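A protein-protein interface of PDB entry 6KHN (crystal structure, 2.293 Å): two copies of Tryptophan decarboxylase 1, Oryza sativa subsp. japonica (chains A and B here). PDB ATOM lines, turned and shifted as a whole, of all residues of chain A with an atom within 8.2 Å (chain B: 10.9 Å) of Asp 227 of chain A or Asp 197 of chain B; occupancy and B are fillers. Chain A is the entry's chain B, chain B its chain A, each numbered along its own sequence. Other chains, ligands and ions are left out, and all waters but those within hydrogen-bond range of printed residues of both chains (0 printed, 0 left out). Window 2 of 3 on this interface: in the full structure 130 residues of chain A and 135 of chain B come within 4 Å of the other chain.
Leu 202 of chain A touches its own counterpart, Leu 202 of chain B. 6 positions are printed for both chains.
Asp 227 of chain A touches three residues of chain B. Of chain A, only Asp 227 (3.9 Å) comes within 4 Å of Asp 197 of chain B. No residue of chain B comes within 4 Å of Ala 229 of chain A. No residue of chain B comes within 4 Å of Asn 230 of chain A. No residue of chain B comes within 4 Å of Ile 231 of chain A. No residue of chain A comes within 4 Å of Ser 196 of chain B. Of the printed residues of chain B, Leu 202 of chain A touches Leu 202. Printed residues of chain B within 4 Å of Arg 222 of chain A: Arg 187. Printed residues of chain A within 4 Å of Arg 187 of chain B: Arg 222 (2.7 Å) and Gly 225 (3.8 Å). Of the printed residues of chain B, His 203 of chain A touches Val 199 (3.9 Å) and Ala 200 (3.8 Å). Of the printed residues of chain A, Ala 200 of chain B touches His 203 (3.8 Å). The nearest residue of chain A that does not touch Asp 197 of chain B is His 203 of chain A (5.1 Å). The nearest printed residue of chain A that does not touch Val 199 of chain B is Leu 202 of chain A (4.1 Å).
Hydrophobic or aromatic side chains of chain A that line the printed part of chain B: Leu 202 and His 203. Of the 21 printed residues of chain B, 6 touch a printed residue of chain A. Hydrophobic or aromatic side chains of chain B within 4 Å of the printed part of chain A: Val 199 and Leu 202.
CD2 of Leu 202 of chain A touches CD2 of Leu 202 of chain B (3.6 Å). Val 199 of chain B touches His 203 of chain A. His 203 of chain A touches Ala 200 of chain B. Gly 225 of chain A touches Arg 187 of chain B (N to NH1, 3.8 Å). Gly 225 of chain A touches Val 199 of chain B. Phe 226 of chain A touches Val 199 of chain B. Asp 227 of chain A touches Asp 197 of chain B (OD2 to O, 3.9 Å). Gly 198 of chain B touches Asp 227 of chain A (CA to OD2, 3.3 Å).
The backbone carbonyl oxygen of His 203 of chain A lies within hydrogen-bond range of the side-chain amide nitrogen of Asn 230 of chain A (2.8 Å). OD1 of Asp 227 of chain A is in hydrogen-bond range of N of Ala 229 of chain A. The backbone carbonyl oxygen (O) of Gly 198 of chain B lies within hydrogen-bond range of the side-chain hydroxyl (OG) of Ser 196 of chain B. N of Phe 226 of chain A is in hydrogen-bond range of O of Cys 221 of chain A (3.1 Å). The backbone carbonyl oxygen (O) of Ala 224 of chain B lies within hydrogen-bond range of the guanidinium group (NH1) of Arg 187 of chain B (2.6 Å). O of Phe 218 of chain A is in hydrogen-bond range of NH1 of Arg 222 of chain A (3.2 Å).
NH2 of Arg 187 of chain B is in hydrogen-bond range of O of Arg 222 of chain A (2.7 Å). The side-chain carboxylate of Asp 227 of chain A is in hydrogen-bond range of the backbone NH of Val 199 of chain B (2.9 Å).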
ATOM      1  N   LEU A 202     -10.216 -33.015  22.639  1.00  0.00           N
ATOM      2  CA  LEU A 202      -9.281 -33.112  23.759  1.00  0.00           C
ATOM      3  C   LEU A 202      -9.726 -32.269  24.954  1.00  0.00           C
ATOM      4  O   LEU A 202      -9.499 -32.660  26.103  1.00  0.00           O
ATOM      5  CB  LEU A 202      -7.886 -32.707  23.279  1.00  0.00           C
ATOM      6  CG  LEU A 202      -6.641 -32.768  24.158  1.00  0.00           C
ATOM      7  CD1 LEU A 202      -6.516 -34.104  24.916  1.00  0.00           C
ATOM      8  CD2 LEU A 202      -5.442 -32.550  23.268  1.00  0.00           C
ATOM      9  N   HIS A 203     -10.411 -31.147  24.714  1.00  0.00           N
ATOM     10  CA  HIS A 203     -10.870 -30.296  25.808  1.00  0.00           C
ATOM     11  C   HIS A 203     -11.977 -30.932  26.649  1.00  0.00           C
ATOM     12  O   HIS A 203     -12.361 -30.355  27.672  1.00  0.00           O
ATOM     13  CB  HIS A 203     -11.352 -28.956  25.264  1.00  0.00           C
ATOM     14  CG  HIS A 203     -12.686 -29.042  24.599  1.00  0.00           C
ATOM     15  ND1 HIS A 203     -12.835 -29.442  23.286  1.00  0.00           N
ATOM     16  CD2 HIS A 203     -13.936 -28.828  25.074  1.00  0.00           C
ATOM     17  CE1 HIS A 203     -14.119 -29.449  22.975  1.00  0.00           C
ATOM     18  NE2 HIS A 203     -14.809 -29.084  24.043  1.00  0.00           N
ATOM     19  N   ARG A 204     -12.492 -32.099  26.265  1.00  0.00           N
ATOM     20  CA  ARG A 204     -13.439 -32.822  27.111  1.00  0.00           C
ATOM     21  C   ARG A 204     -12.792 -33.913  27.977  1.00  0.00           C
ATOM     22  O   ARG A 204     -13.474 -34.483  28.835  1.00  0.00           O
ATOM     23  CB  ARG A 204     -14.533 -33.451  26.241  1.00  0.00           C
ATOM     24  CG  ARG A 204     -15.061 -32.537  25.117  1.00  0.00           C
ATOM     25  CD  ARG A 204     -16.158 -33.222  24.295  1.00  0.00           C
ATOM     26  NE  ARG A 204     -16.985 -34.086  25.140  1.00  0.00           N
ATOM     27  CZ  ARG A 204     -17.488 -35.256  24.752  1.00  0.00           C
ATOM     28  NH1 ARG A 204     -17.253 -35.706  23.520  1.00  0.00           N
ATOM     29  NH2 ARG A 204     -18.223 -35.980  25.599  1.00  0.00           N
ATOM     30  N   LEU A 205     -11.514 -34.238  27.787  1.00  0.00           N
ATOM     31  CA  LEU A 205     -10.911 -35.316  28.572  1.00  0.00           C
ATOM     32  C   LEU A 205     -10.478 -34.809  29.943  1.00  0.00           C
ATOM     33  O   LEU A 205      -9.890 -33.727  30.065  1.00  0.00           O
ATOM     34  CB  LEU A 205      -9.713 -35.920  27.836  1.00  0.00           C
ATOM     35  CG  LEU A 205      -9.899 -36.343  26.375  1.00  0.00           C
ATOM     36  CD1 LEU A 205      -8.695 -37.113  25.881  1.00  0.00           C
ATOM     37  CD2 LEU A 205     -11.174 -37.159  26.184  1.00  0.00           C
ATOM     38  N   ALA A 206     -10.775 -35.592  30.980  1.00  0.00           N
ATOM     39  CA  ALA A 206     -10.404 -35.266  32.353  1.00  0.00           C
ATOM     40  C   ALA A 206      -9.499 -36.348  32.935  1.00  0.00           C
ATOM     41  O   ALA A 206      -9.569 -37.516  32.546  1.00  0.00           O
ATOM     42  CB  ALA A 206     -11.642 -35.094  33.237  1.00  0.00           C
ATOM     43  N   VAL A 207      -8.647 -35.944  33.883  1.00  0.00           N
ATOM     44  CA  VAL A 207      -7.647 -36.806  34.503  1.00  0.00           C
ATOM     45  C   VAL A 207      -7.636 -36.536  36.001  1.00  0.00           C
ATOM     46  O   VAL A 207      -7.991 -35.441  36.449  1.00  0.00           O
ATOM     47  CB  VAL A 207      -6.250 -36.576  33.892  1.00  0.00           C
ATOM     48  CG1 VAL A 207      -6.229 -37.056  32.452  1.00  0.00           C
ATOM     49  CG2 VAL A 207      -5.897 -35.112  33.938  1.00  0.00           C
ATOM     50  N   PHE A 218       1.095 -33.946  37.309  1.00  0.00           N
ATOM     51  CA  PHE A 218       0.236 -32.910  36.743  1.00  0.00           C
ATOM     52  C   PHE A 218       0.949 -32.157  35.631  1.00  0.00           C
ATOM     53  O   PHE A 218       0.303 -31.739  34.661  1.00  0.00           O
ATOM     54  CB  PHE A 218      -0.247 -31.979  37.858  1.00  0.00           C
ATOM     55  CG  PHE A 218      -0.868 -32.732  39.019  1.00  0.00           C
ATOM     56  CD1 PHE A 218      -2.200 -33.130  38.973  1.00  0.00           C
ATOM     57  CD2 PHE A 218      -0.108 -33.093  40.122  1.00  0.00           C
ATOM     58  CE1 PHE A 218      -2.770 -33.841  40.020  1.00  0.00           C
ATOM     59  CE2 PHE A 218      -0.674 -33.805  41.187  1.00  0.00           C
ATOM     60  CZ  PHE A 218      -2.002 -34.188  41.133  1.00  0.00           C
ATOM     61  N   CYS A 221       0.522 -34.359  32.588  1.00  0.00           N
ATOM     62  CA  CYS A 221      -0.815 -34.128  32.039  1.00  0.00           C
ATOM     63  C   CYS A 221      -0.838 -32.925  31.105  1.00  0.00           C
ATOM     64  O   CYS A 221      -1.413 -32.984  30.013  1.00  0.00           O
ATOM     65  CB  CYS A 221      -1.815 -33.934  33.171  1.00  0.00           C
ATOM     66  SG  CYS A 221      -2.083 -35.407  34.145  1.00  0.00           S
ATOM     67  N   ARG A 222      -0.213 -31.818  31.521  1.00  0.00           N
ATOM     68  CA  ARG A 222      -0.196 -30.622  30.682  1.00  0.00           C
ATOM     69  C   ARG A 222       0.673 -30.826  29.448  1.00  0.00           C
ATOM     70  O   ARG A 222       0.355 -30.308  28.378  1.00  0.00           O
ATOM     71  CB  ARG A 222       0.286 -29.410  31.489  1.00  0.00           C
ATOM     72  CG  ARG A 222      -0.584 -29.105  32.700  1.00  0.00           C
ATOM     73  CD  ARG A 222      -0.240 -27.752  33.335  1.00  0.00           C
ATOM     74  NE  ARG A 222       1.060 -27.758  34.005  1.00  0.00           N
ATOM     75  CZ  ARG A 222       1.289 -28.274  35.213  1.00  0.00           C
ATOM     76  NH1 ARG A 222       0.300 -28.829  35.911  1.00  0.00           N
ATOM     77  NH2 ARG A 222       2.508 -28.226  35.730  1.00  0.00           N
ATOM     78  N   ALA A 224       1.005 -33.635  27.839  1.00  0.00           N
ATOM     79  CA  ALA A 224       0.214 -34.462  26.941  1.00  0.00           C
ATOM     80  C   ALA A 224      -0.947 -33.704  26.308  1.00  0.00           C
ATOM     81  O   ALA A 224      -1.626 -34.264  25.446  1.00  0.00           O
ATOM     82  CB  ALA A 224      -0.312 -35.691  27.684  1.00  0.00           C
ATOM     83  N   GLY A 225      -1.195 -32.460  26.716  1.00  0.00           N
ATOM     84  CA  GLY A 225      -2.207 -31.635  26.090  1.00  0.00           C
ATOM     85  C   GLY A 225      -3.538 -31.586  26.812  1.00  0.00           C
ATOM     86  O   GLY A 225      -4.462 -30.934  26.321  1.00  0.00           O
ATOM     87  N   PHE A 226      -3.668 -32.247  27.957  1.00  0.00           N
ATOM     88  CA  PHE A 226      -4.889 -32.115  28.732  1.00  0.00           C
ATOM     89  C   PHE A 226      -5.104 -30.665  29.158  1.00  0.00           C
ATOM     90  O   PHE A 226      -4.164 -29.871  29.284  1.00  0.00           O
ATOM     91  CB  PHE A 226      -4.850 -33.036  29.957  1.00  0.00           C
ATOM     92  CG  PHE A 226      -4.946 -34.497  29.608  1.00  0.00           C
ATOM     93  CD1 PHE A 226      -6.181 -35.096  29.424  1.00  0.00           C
ATOM     94  CD2 PHE A 226      -3.802 -35.261  29.430  1.00  0.00           C
ATOM     95  CE1 PHE A 226      -6.274 -36.436  29.076  1.00  0.00           C
ATOM     96  CE2 PHE A 226      -3.882 -36.603  29.090  1.00  0.00           C
ATOM     97  CZ  PHE A 226      -5.116 -37.198  28.921  1.00  0.00           C
ATOM     98  N   ASP A 227      -6.356 -30.332  29.371  1.00  0.00           N
ATOM     99  CA  ASP A 227      -6.751 -28.974  29.683  1.00  0.00           C
ATOM    100  C   ASP A 227      -6.554 -28.719  31.171  1.00  0.00           C
ATOM    101  O   ASP A 227      -7.032 -29.509  31.985  1.00  0.00           O
ATOM    102  CB  ASP A 227      -8.215 -28.774  29.301  1.00  0.00           C
ATOM    103  CG  ASP A 227      -8.607 -27.320  29.212  1.00  0.00           C
ATOM    104  OD1 ASP A 227      -8.468 -26.592  30.228  1.00  0.00           O
ATOM    105  OD2 ASP A 227      -9.073 -26.912  28.116  1.00  0.00           O
ATOM    106  N   PRO A 228      -5.851 -27.641  31.559  1.00  0.00           N
ATOM    107  CA  PRO A 228      -5.717 -27.308  32.996  1.00  0.00           C
ATOM    108  C   PRO A 228      -7.021 -27.356  33.782  1.00  0.00           C
ATOM    109  O   PRO A 228      -7.027 -27.805  34.937  1.00  0.00           O
ATOM    110  CB  PRO A 228      -5.138 -25.888  32.957  1.00  0.00           C
ATOM    111  CG  PRO A 228      -4.302 -25.894  31.725  1.00  0.00           C
ATOM    112  CD  PRO A 228      -5.053 -26.738  30.714  1.00  0.00           C
ATOM    113  N   ALA A 229      -8.129 -26.919  33.184  1.00  0.00           N
ATOM    114  CA  ALA A 229      -9.417 -26.972  33.866  1.00  0.00           C
ATOM    115  C   ALA A 229      -9.871 -28.393  34.170  1.00  0.00           C
ATOM    116  O   ALA A 229     -10.704 -28.577  35.066  1.00  0.00           O
ATOM    117  CB  ALA A 229     -10.488 -26.273  33.021  1.00  0.00           C
ATOM    118  N   ASN A 230      -9.361 -29.400  33.449  1.00  0.00           N
ATOM    119  CA  ASN A 230      -9.823 -30.780  33.605  1.00  0.00           C
ATOM    120  C   ASN A 230      -8.810 -31.688  34.295  1.00  0.00           C
ATOM    121  O   ASN A 230      -9.005 -32.909  34.317  1.00  0.00           O
ATOM    122  CB  ASN A 230     -10.202 -31.366  32.240  1.00  0.00           C
ATOM    123  CG  ASN A 230     -11.300 -30.570  31.558  1.00  0.00           C
ATOM    124  OD1 ASN A 230     -12.015 -29.810  32.210  1.00  0.00           O
ATOM    125  ND2 ASN A 230     -11.432 -30.732  30.247  1.00  0.00           N
ATOM    126  N   ILE A 231      -7.742 -31.136  34.857  1.00  0.00           N
ATOM    127  CA  ILE A 231      -6.739 -31.910  35.585  1.00  0.00           C
ATOM    128  C   ILE A 231      -7.092 -31.821  37.064  1.00  0.00           C
ATOM    129  O   ILE A 231      -6.964 -30.754  37.670  1.00  0.00           O
ATOM    130  CB  ILE A 231      -5.322 -31.392  35.301  1.00  0.00           C
ATOM    131  CG1 ILE A 231      -5.061 -31.411  33.794  1.00  0.00           C
ATOM    132  CG2 ILE A 231      -4.276 -32.225  36.044  1.00  0.00           C
ATOM    133  CD1 ILE A 231      -3.805 -30.658  33.354  1.00  0.00           C
ATOM    134  N   ARG A 232      -7.566 -32.919  37.648  1.00  0.00           N
ATOM    135  CA  ARG A 232      -8.114 -32.910  39.000  1.00  0.00           C
ATOM    136  C   ARG A 232      -7.074 -33.359  40.020  1.00  0.00           C
ATOM    137  O   ARG A 232      -6.500 -34.445  39.894  1.00  0.00           O
ATOM    138  CB  ARG A 232      -9.337 -33.819  39.115  1.00  0.00           C
ATOM    139  CG  ARG A 232     -10.337 -33.643  38.016  1.00  0.00           C
ATOM    140  CD  ARG A 232     -11.331 -32.598  38.382  1.00  0.00           C
ATOM    141  NE  ARG A 232     -12.274 -32.378  37.292  1.00  0.00           N
ATOM    142  CZ  ARG A 232     -12.382 -31.239  36.625  1.00  0.00           C
ATOM    143  NH1 ARG A 232     -11.598 -30.209  36.927  1.00  0.00           N
ATOM    144  NH2 ARG A 232     -13.268 -31.135  35.648  1.00  0.00           N
ATOM    145  N   LEU A 261     -17.999 -34.381  30.417  1.00  0.00           N
ATOM    146  CA  LEU A 261     -16.572 -34.625  30.234  1.00  0.00           C
ATOM    147  C   LEU A 261     -16.291 -36.129  30.180  1.00  0.00           C
ATOM    148  O   LEU A 261     -17.127 -36.952  30.563  1.00  0.00           O
ATOM    149  CB  LEU A 261     -15.770 -33.968  31.363  1.00  0.00           C
ATOM    150  CG  LEU A 261     -15.913 -32.446  31.497  1.00  0.00           C
ATOM    151  CD1 LEU A 261     -15.253 -31.959  32.772  1.00  0.00           C
ATOM    152  CD2 LEU A 261     -15.344 -31.721  30.284  1.00  0.00           C
ATOM    153  N   ARG B 187       3.830 -24.615  21.519  1.00  0.00           N
ATOM    154  CA  ARG B 187       2.393 -24.855  21.589  1.00  0.00           C
ATOM    155  C   ARG B 187       1.739 -23.933  22.606  1.00  0.00           C
ATOM    156  O   ARG B 187       0.735 -23.277  22.309  1.00  0.00           O
ATOM    157  CB  ARG B 187       2.120 -26.319  21.949  1.00  0.00           C
ATOM    158  CG  ARG B 187       0.648 -26.650  22.175  1.00  0.00           C
ATOM    159  CD  ARG B 187       0.495 -27.976  22.914  1.00  0.00           C
ATOM    160  NE  ARG B 187       0.745 -27.811  24.348  1.00  0.00           N
ATOM    161  CZ  ARG B 187       0.991 -28.803  25.203  1.00  0.00           C
ATOM    162  NH1 ARG B 187       1.010 -30.064  24.787  1.00  0.00           N
ATOM    163  NH2 ARG B 187       1.194 -28.531  26.488  1.00  0.00           N
ATOM    164  N   ASP B 188       2.310 -23.860  23.809  1.00  0.00           N
ATOM    165  CA  ASP B 188       1.689 -23.076  24.868  1.00  0.00           C
ATOM    166  C   ASP B 188       1.673 -21.591  24.521  1.00  0.00           C
ATOM    167  O   ASP B 188       0.701 -20.895  24.837  1.00  0.00           O
ATOM    168  CB  ASP B 188       2.403 -23.325  26.201  1.00  0.00           C
ATOM    169  CG  ASP B 188       2.226 -24.786  26.709  1.00  0.00           C
ATOM    170  OD1 ASP B 188       1.297 -25.494  26.228  1.00  0.00           O
ATOM    171  OD2 ASP B 188       3.011 -25.233  27.594  1.00  0.00           O
ATOM    172  N   ALA B 190       1.523 -20.394  21.408  1.00  0.00           N
ATOM    173  CA  ALA B 190       0.536 -20.221  20.345  1.00  0.00           C
ATOM    174  C   ALA B 190      -0.886 -20.267  20.898  1.00  0.00           C
ATOM    175  O   ALA B 190      -1.727 -19.428  20.553  1.00  0.00           O
ATOM    176  CB  ALA B 190       0.733 -21.278  19.257  1.00  0.00           C
ATOM    177  N   LEU B 191      -1.177 -21.234  21.765  1.00  0.00           N
ATOM    178  CA  LEU B 191      -2.503 -21.290  22.377  1.00  0.00           C
ATOM    179  C   LEU B 191      -2.807 -20.005  23.141  1.00  0.00           C
ATOM    180  O   LEU B 191      -3.919 -19.472  23.062  1.00  0.00           O
ATOM    181  CB  LEU B 191      -2.604 -22.497  23.314  1.00  0.00           C
ATOM    182  CG  LEU B 191      -2.683 -23.883  22.662  1.00  0.00           C
ATOM    183  CD1 LEU B 191      -2.734 -24.975  23.733  1.00  0.00           C
ATOM    184  CD2 LEU B 191      -3.879 -23.980  21.701  1.00  0.00           C
ATOM    185  N   ARG B 192      -1.823 -19.498  23.884  1.00  0.00           N
ATOM    186  CA  ARG B 192      -2.039 -18.300  24.685  1.00  0.00           C
ATOM    187  C   ARG B 192      -2.383 -17.098  23.807  1.00  0.00           C
ATOM    188  O   ARG B 192      -3.387 -16.417  24.036  1.00  0.00           O
ATOM    189  CB  ARG B 192      -0.797 -18.012  25.522  1.00  0.00           C
ATOM    190  CG  ARG B 192      -0.991 -16.900  26.512  1.00  0.00           C
ATOM    191  CD  ARG B 192       0.331 -16.316  26.968  1.00  0.00           C
ATOM    192  NE  ARG B 192       1.258 -17.346  27.402  1.00  0.00           N
ATOM    193  CZ  ARG B 192       2.500 -17.488  26.933  1.00  0.00           C
ATOM    194  NH1 ARG B 192       2.987 -16.646  26.017  1.00  0.00           N
ATOM    195  NH2 ARG B 192       3.257 -18.479  27.402  1.00  0.00           N
ATOM    196  N   ARG B 193      -1.564 -16.827  22.794  1.00  0.00           N
ATOM    197  CA  ARG B 193      -1.718 -15.588  22.054  1.00  0.00           C
ATOM    198  C   ARG B 193      -2.843 -15.650  21.031  1.00  0.00           C
ATOM    199  O   ARG B 193      -3.358 -14.597  20.641  1.00  0.00           O
ATOM    200  CB  ARG B 193      -0.402 -15.210  21.372  1.00  0.00           C
ATOM    201  CG  ARG B 193      -0.022 -16.104  20.233  1.00  0.00           C
ATOM    202  CD  ARG B 193       1.312 -15.677  19.613  1.00  0.00           C
ATOM    203  NE  ARG B 193       2.384 -15.442  20.591  1.00  0.00           N
ATOM    204  CZ  ARG B 193       3.568 -16.058  20.572  1.00  0.00           C
ATOM    205  NH1 ARG B 193       3.834 -16.969  19.631  1.00  0.00           N
ATOM    206  NH2 ARG B 193       4.487 -15.763  21.490  1.00  0.00           N
ATOM    207  N   SER B 194      -3.257 -16.843  20.613  1.00  0.00           N
ATOM    208  CA  SER B 194      -4.341 -16.983  19.652  1.00  0.00           C
ATOM    209  C   SER B 194      -5.695 -17.198  20.315  1.00  0.00           C
ATOM    210  O   SER B 194      -6.653 -17.552  19.627  1.00  0.00           O
ATOM    211  CB  SER B 194      -4.046 -18.126  18.679  1.00  0.00           C
ATOM    212  OG  SER B 194      -4.286 -19.371  19.294  1.00  0.00           O
ATOM    213  N   GLY B 195      -5.797 -16.995  21.627  1.00  0.00           N
ATOM    214  CA  GLY B 195      -7.095 -16.982  22.276  1.00  0.00           C
ATOM    215  C   GLY B 195      -7.767 -18.330  22.426  1.00  0.00           C
ATOM    216  O   GLY B 195      -9.000 -18.402  22.430  1.00  0.00           O
ATOM    217  N   SER B 196      -6.995 -19.404  22.566  1.00  0.00           N
ATOM    218  CA  SER B 196      -7.603 -20.707  22.808  1.00  0.00           C
ATOM    219  C   SER B 196      -8.343 -20.711  24.140  1.00  0.00           C
ATOM    220  O   SER B 196      -7.891 -20.130  25.132  1.00  0.00           O
ATOM    221  CB  SER B 196      -6.542 -21.809  22.800  1.00  0.00           C
ATOM    222  OG  SER B 196      -7.123 -23.085  23.062  1.00  0.00           O
ATOM    223  N   ASP B 197      -9.505 -21.356  24.152  1.00  0.00           N
ATOM    224  CA  ASP B 197     -10.236 -21.622  25.389  1.00  0.00           C
ATOM    225  C   ASP B 197      -9.661 -22.916  25.970  1.00  0.00           C
ATOM    226  O   ASP B 197     -10.078 -24.024  25.619  1.00  0.00           O
ATOM    227  CB  ASP B 197     -11.737 -21.713  25.116  1.00  0.00           C
ATOM    228  CG  ASP B 197     -12.263 -20.554  24.220  1.00  0.00           C
ATOM    229  OD1 ASP B 197     -11.680 -19.442  24.239  1.00  0.00           O
ATOM    230  OD2 ASP B 197     -13.266 -20.755  23.497  1.00  0.00           O
ATOM    231  N   GLY B 198      -8.668 -22.778  26.853  1.00  0.00           N
ATOM    232  CA  GLY B 198      -7.933 -23.956  27.291  1.00  0.00           C
ATOM    233  C   GLY B 198      -7.235 -24.591  26.099  1.00  0.00           C
ATOM    234  O   GLY B 198      -6.561 -23.904  25.322  1.00  0.00           O
ATOM    235  N   VAL B 199      -7.410 -25.906  25.926  1.00  0.00           N
ATOM    236  CA  VAL B 199      -6.855 -26.612  24.769  1.00  0.00           C
ATOM    237  C   VAL B 199      -7.897 -26.833  23.667  1.00  0.00           C
ATOM    238  O   VAL B 199      -7.610 -27.532  22.687  1.00  0.00           O
ATOM    239  CB  VAL B 199      -6.202 -27.953  25.163  1.00  0.00           C
ATOM    240  CG1 VAL B 199      -5.135 -27.757  26.261  1.00  0.00           C
ATOM    241  CG2 VAL B 199      -7.259 -28.979  25.569  1.00  0.00           C
ATOM    242  N   ALA B 200      -9.096 -26.246  23.795  1.00  0.00           N
ATOM    243  CA  ALA B 200     -10.080 -26.334  22.710  1.00  0.00           C
ATOM    244  C   ALA B 200      -9.496 -25.883  21.374  1.00  0.00           C
ATOM    245  O   ALA B 200      -9.862 -26.422  20.326  1.00  0.00           O
ATOM    246  CB  ALA B 200     -11.333 -25.513  23.047  1.00  0.00           C
ATOM    247  N   GLY B 201      -8.576 -24.919  21.386  1.00  0.00           N
ATOM    248  CA  GLY B 201      -7.960 -24.471  20.152  1.00  0.00           C
ATOM    249  C   GLY B 201      -6.761 -25.266  19.683  1.00  0.00           C
ATOM    250  O   GLY B 201      -6.157 -24.885  18.673  1.00  0.00           O
ATOM    251  N   LEU B 202      -6.397 -26.359  20.374  1.00  0.00           N
ATOM    252  CA  LEU B 202      -5.207 -27.123  19.997  1.00  0.00           C
ATOM    253  C   LEU B 202      -5.338 -27.711  18.599  1.00  0.00           C
ATOM    254  O   LEU B 202      -4.344 -27.817  17.872  1.00  0.00           O
ATOM    255  CB  LEU B 202      -4.939 -28.240  21.017  1.00  0.00           C
ATOM    256  CG  LEU B 202      -3.638 -29.060  20.961  1.00  0.00           C
ATOM    257  CD1 LEU B 202      -2.421 -28.225  20.590  1.00  0.00           C
ATOM    258  CD2 LEU B 202      -3.386 -29.745  22.293  1.00  0.00           C
ATOM    259  N   HIS B 203      -6.545 -28.080  18.196  1.00  0.00           N
ATOM    260  CA  HIS B 203      -6.709 -28.614  16.850  1.00  0.00           C
ATOM    261  C   HIS B 203      -6.490 -27.572  15.754  1.00  0.00           C
ATOM    262  O   HIS B 203      -6.519 -27.946  14.583  1.00  0.00           O
ATOM    263  CB  HIS B 203      -8.097 -29.229  16.690  1.00  0.00           C
ATOM    264  CG  HIS B 203      -9.169 -28.212  16.493  1.00  0.00           C
ATOM    265  ND1 HIS B 203      -9.827 -27.618  17.548  1.00  0.00           N
ATOM    266  CD2 HIS B 203      -9.668 -27.649  15.369  1.00  0.00           C
ATOM    267  CE1 HIS B 203     -10.699 -26.743  17.081  1.00  0.00           C
ATOM    268  NE2 HIS B 203     -10.619 -26.739  15.762  1.00  0.00           N
ATOM    269  N   ARG B 204      -6.262 -26.298  16.084  1.00  0.00           N
ATOM    270  CA  ARG B 204      -6.004 -25.273  15.076  1.00  0.00           C
ATOM    271  C   ARG B 204      -4.519 -24.991  14.850  1.00  0.00           C
ATOM    272  O   ARG B 204      -4.185 -24.195  13.967  1.00  0.00           O
ATOM    273  CB  ARG B 204      -6.701 -23.960  15.464  1.00  0.00           C
ATOM    274  CG  ARG B 204      -8.213 -23.937  15.234  1.00  0.00           C
ATOM    275  CD  ARG B 204      -8.708 -22.497  15.005  1.00  0.00           C
ATOM    276  NE  ARG B 204      -8.100 -21.537  15.938  1.00  0.00           N
ATOM    277  CZ  ARG B 204      -7.823 -20.258  15.655  1.00  0.00           C
ATOM    278  NH1 ARG B 204      -8.087 -19.752  14.451  1.00  0.00           N
ATOM    279  NH2 ARG B 204      -7.272 -19.476  16.584  1.00  0.00           N
ATOM    280  N   LEU B 205      -3.619 -25.597  15.618  1.00  0.00           N
ATOM    281  CA  LEU B 205      -2.201 -25.295  15.469  1.00  0.00           C
ATOM    282  C   LEU B 205      -1.600 -26.178  14.393  1.00  0.00           C
ATOM    283  O   LEU B 205      -2.003 -27.327  14.222  1.00  0.00           O
ATOM    284  CB  LEU B 205      -1.458 -25.508  16.785  1.00  0.00           C
ATOM    285  CG  LEU B 205      -2.029 -24.808  18.015  1.00  0.00           C
ATOM    286  CD1 LEU B 205      -1.051 -24.937  19.164  1.00  0.00           C
ATOM    287  CD2 LEU B 205      -2.341 -23.350  17.725  1.00  0.00           C
ATOM    288  N   ALA B 224       2.913 -34.168  22.003  1.00  0.00           N
ATOM    289  CA  ALA B 224       2.494 -32.851  22.484  1.00  0.00           C
ATOM    290  C   ALA B 224       1.031 -32.533  22.203  1.00  0.00           C
ATOM    291  O   ALA B 224       0.553 -31.480  22.642  1.00  0.00           O
ATOM    292  CB  ALA B 224       3.362 -31.743  21.863  1.00  0.00           C
ATOM    293  N   GLY B 225       0.309 -33.391  21.494  1.00  0.00           N
ATOM    294  CA  GLY B 225      -1.103 -33.147  21.252  1.00  0.00           C
ATOM    295  C   GLY B 225      -1.435 -32.422  19.964  1.00  0.00           C
ATOM    296  O   GLY B 225      -2.592 -32.033  19.776  1.00  0.00           O
ATOM    297  N   VAL B 262      -3.137 -21.842  12.863  1.00  0.00           N
ATOM    298  CA  VAL B 262      -2.067 -21.070  13.477  1.00  0.00           C
ATOM    299  C   VAL B 262      -0.749 -21.793  13.244  1.00  0.00           C
ATOM    300  O   VAL B 262      -0.444 -22.779  13.918  1.00  0.00           O
ATOM    301  CB  VAL B 262      -2.310 -20.857  14.981  1.00  0.00           C
ATOM    302  CG1 VAL B 262      -1.201 -19.983  15.564  1.00  0.00           C
ATOM    303  CG2 VAL B 262      -3.698 -20.270  15.234  1.00  0.00           C
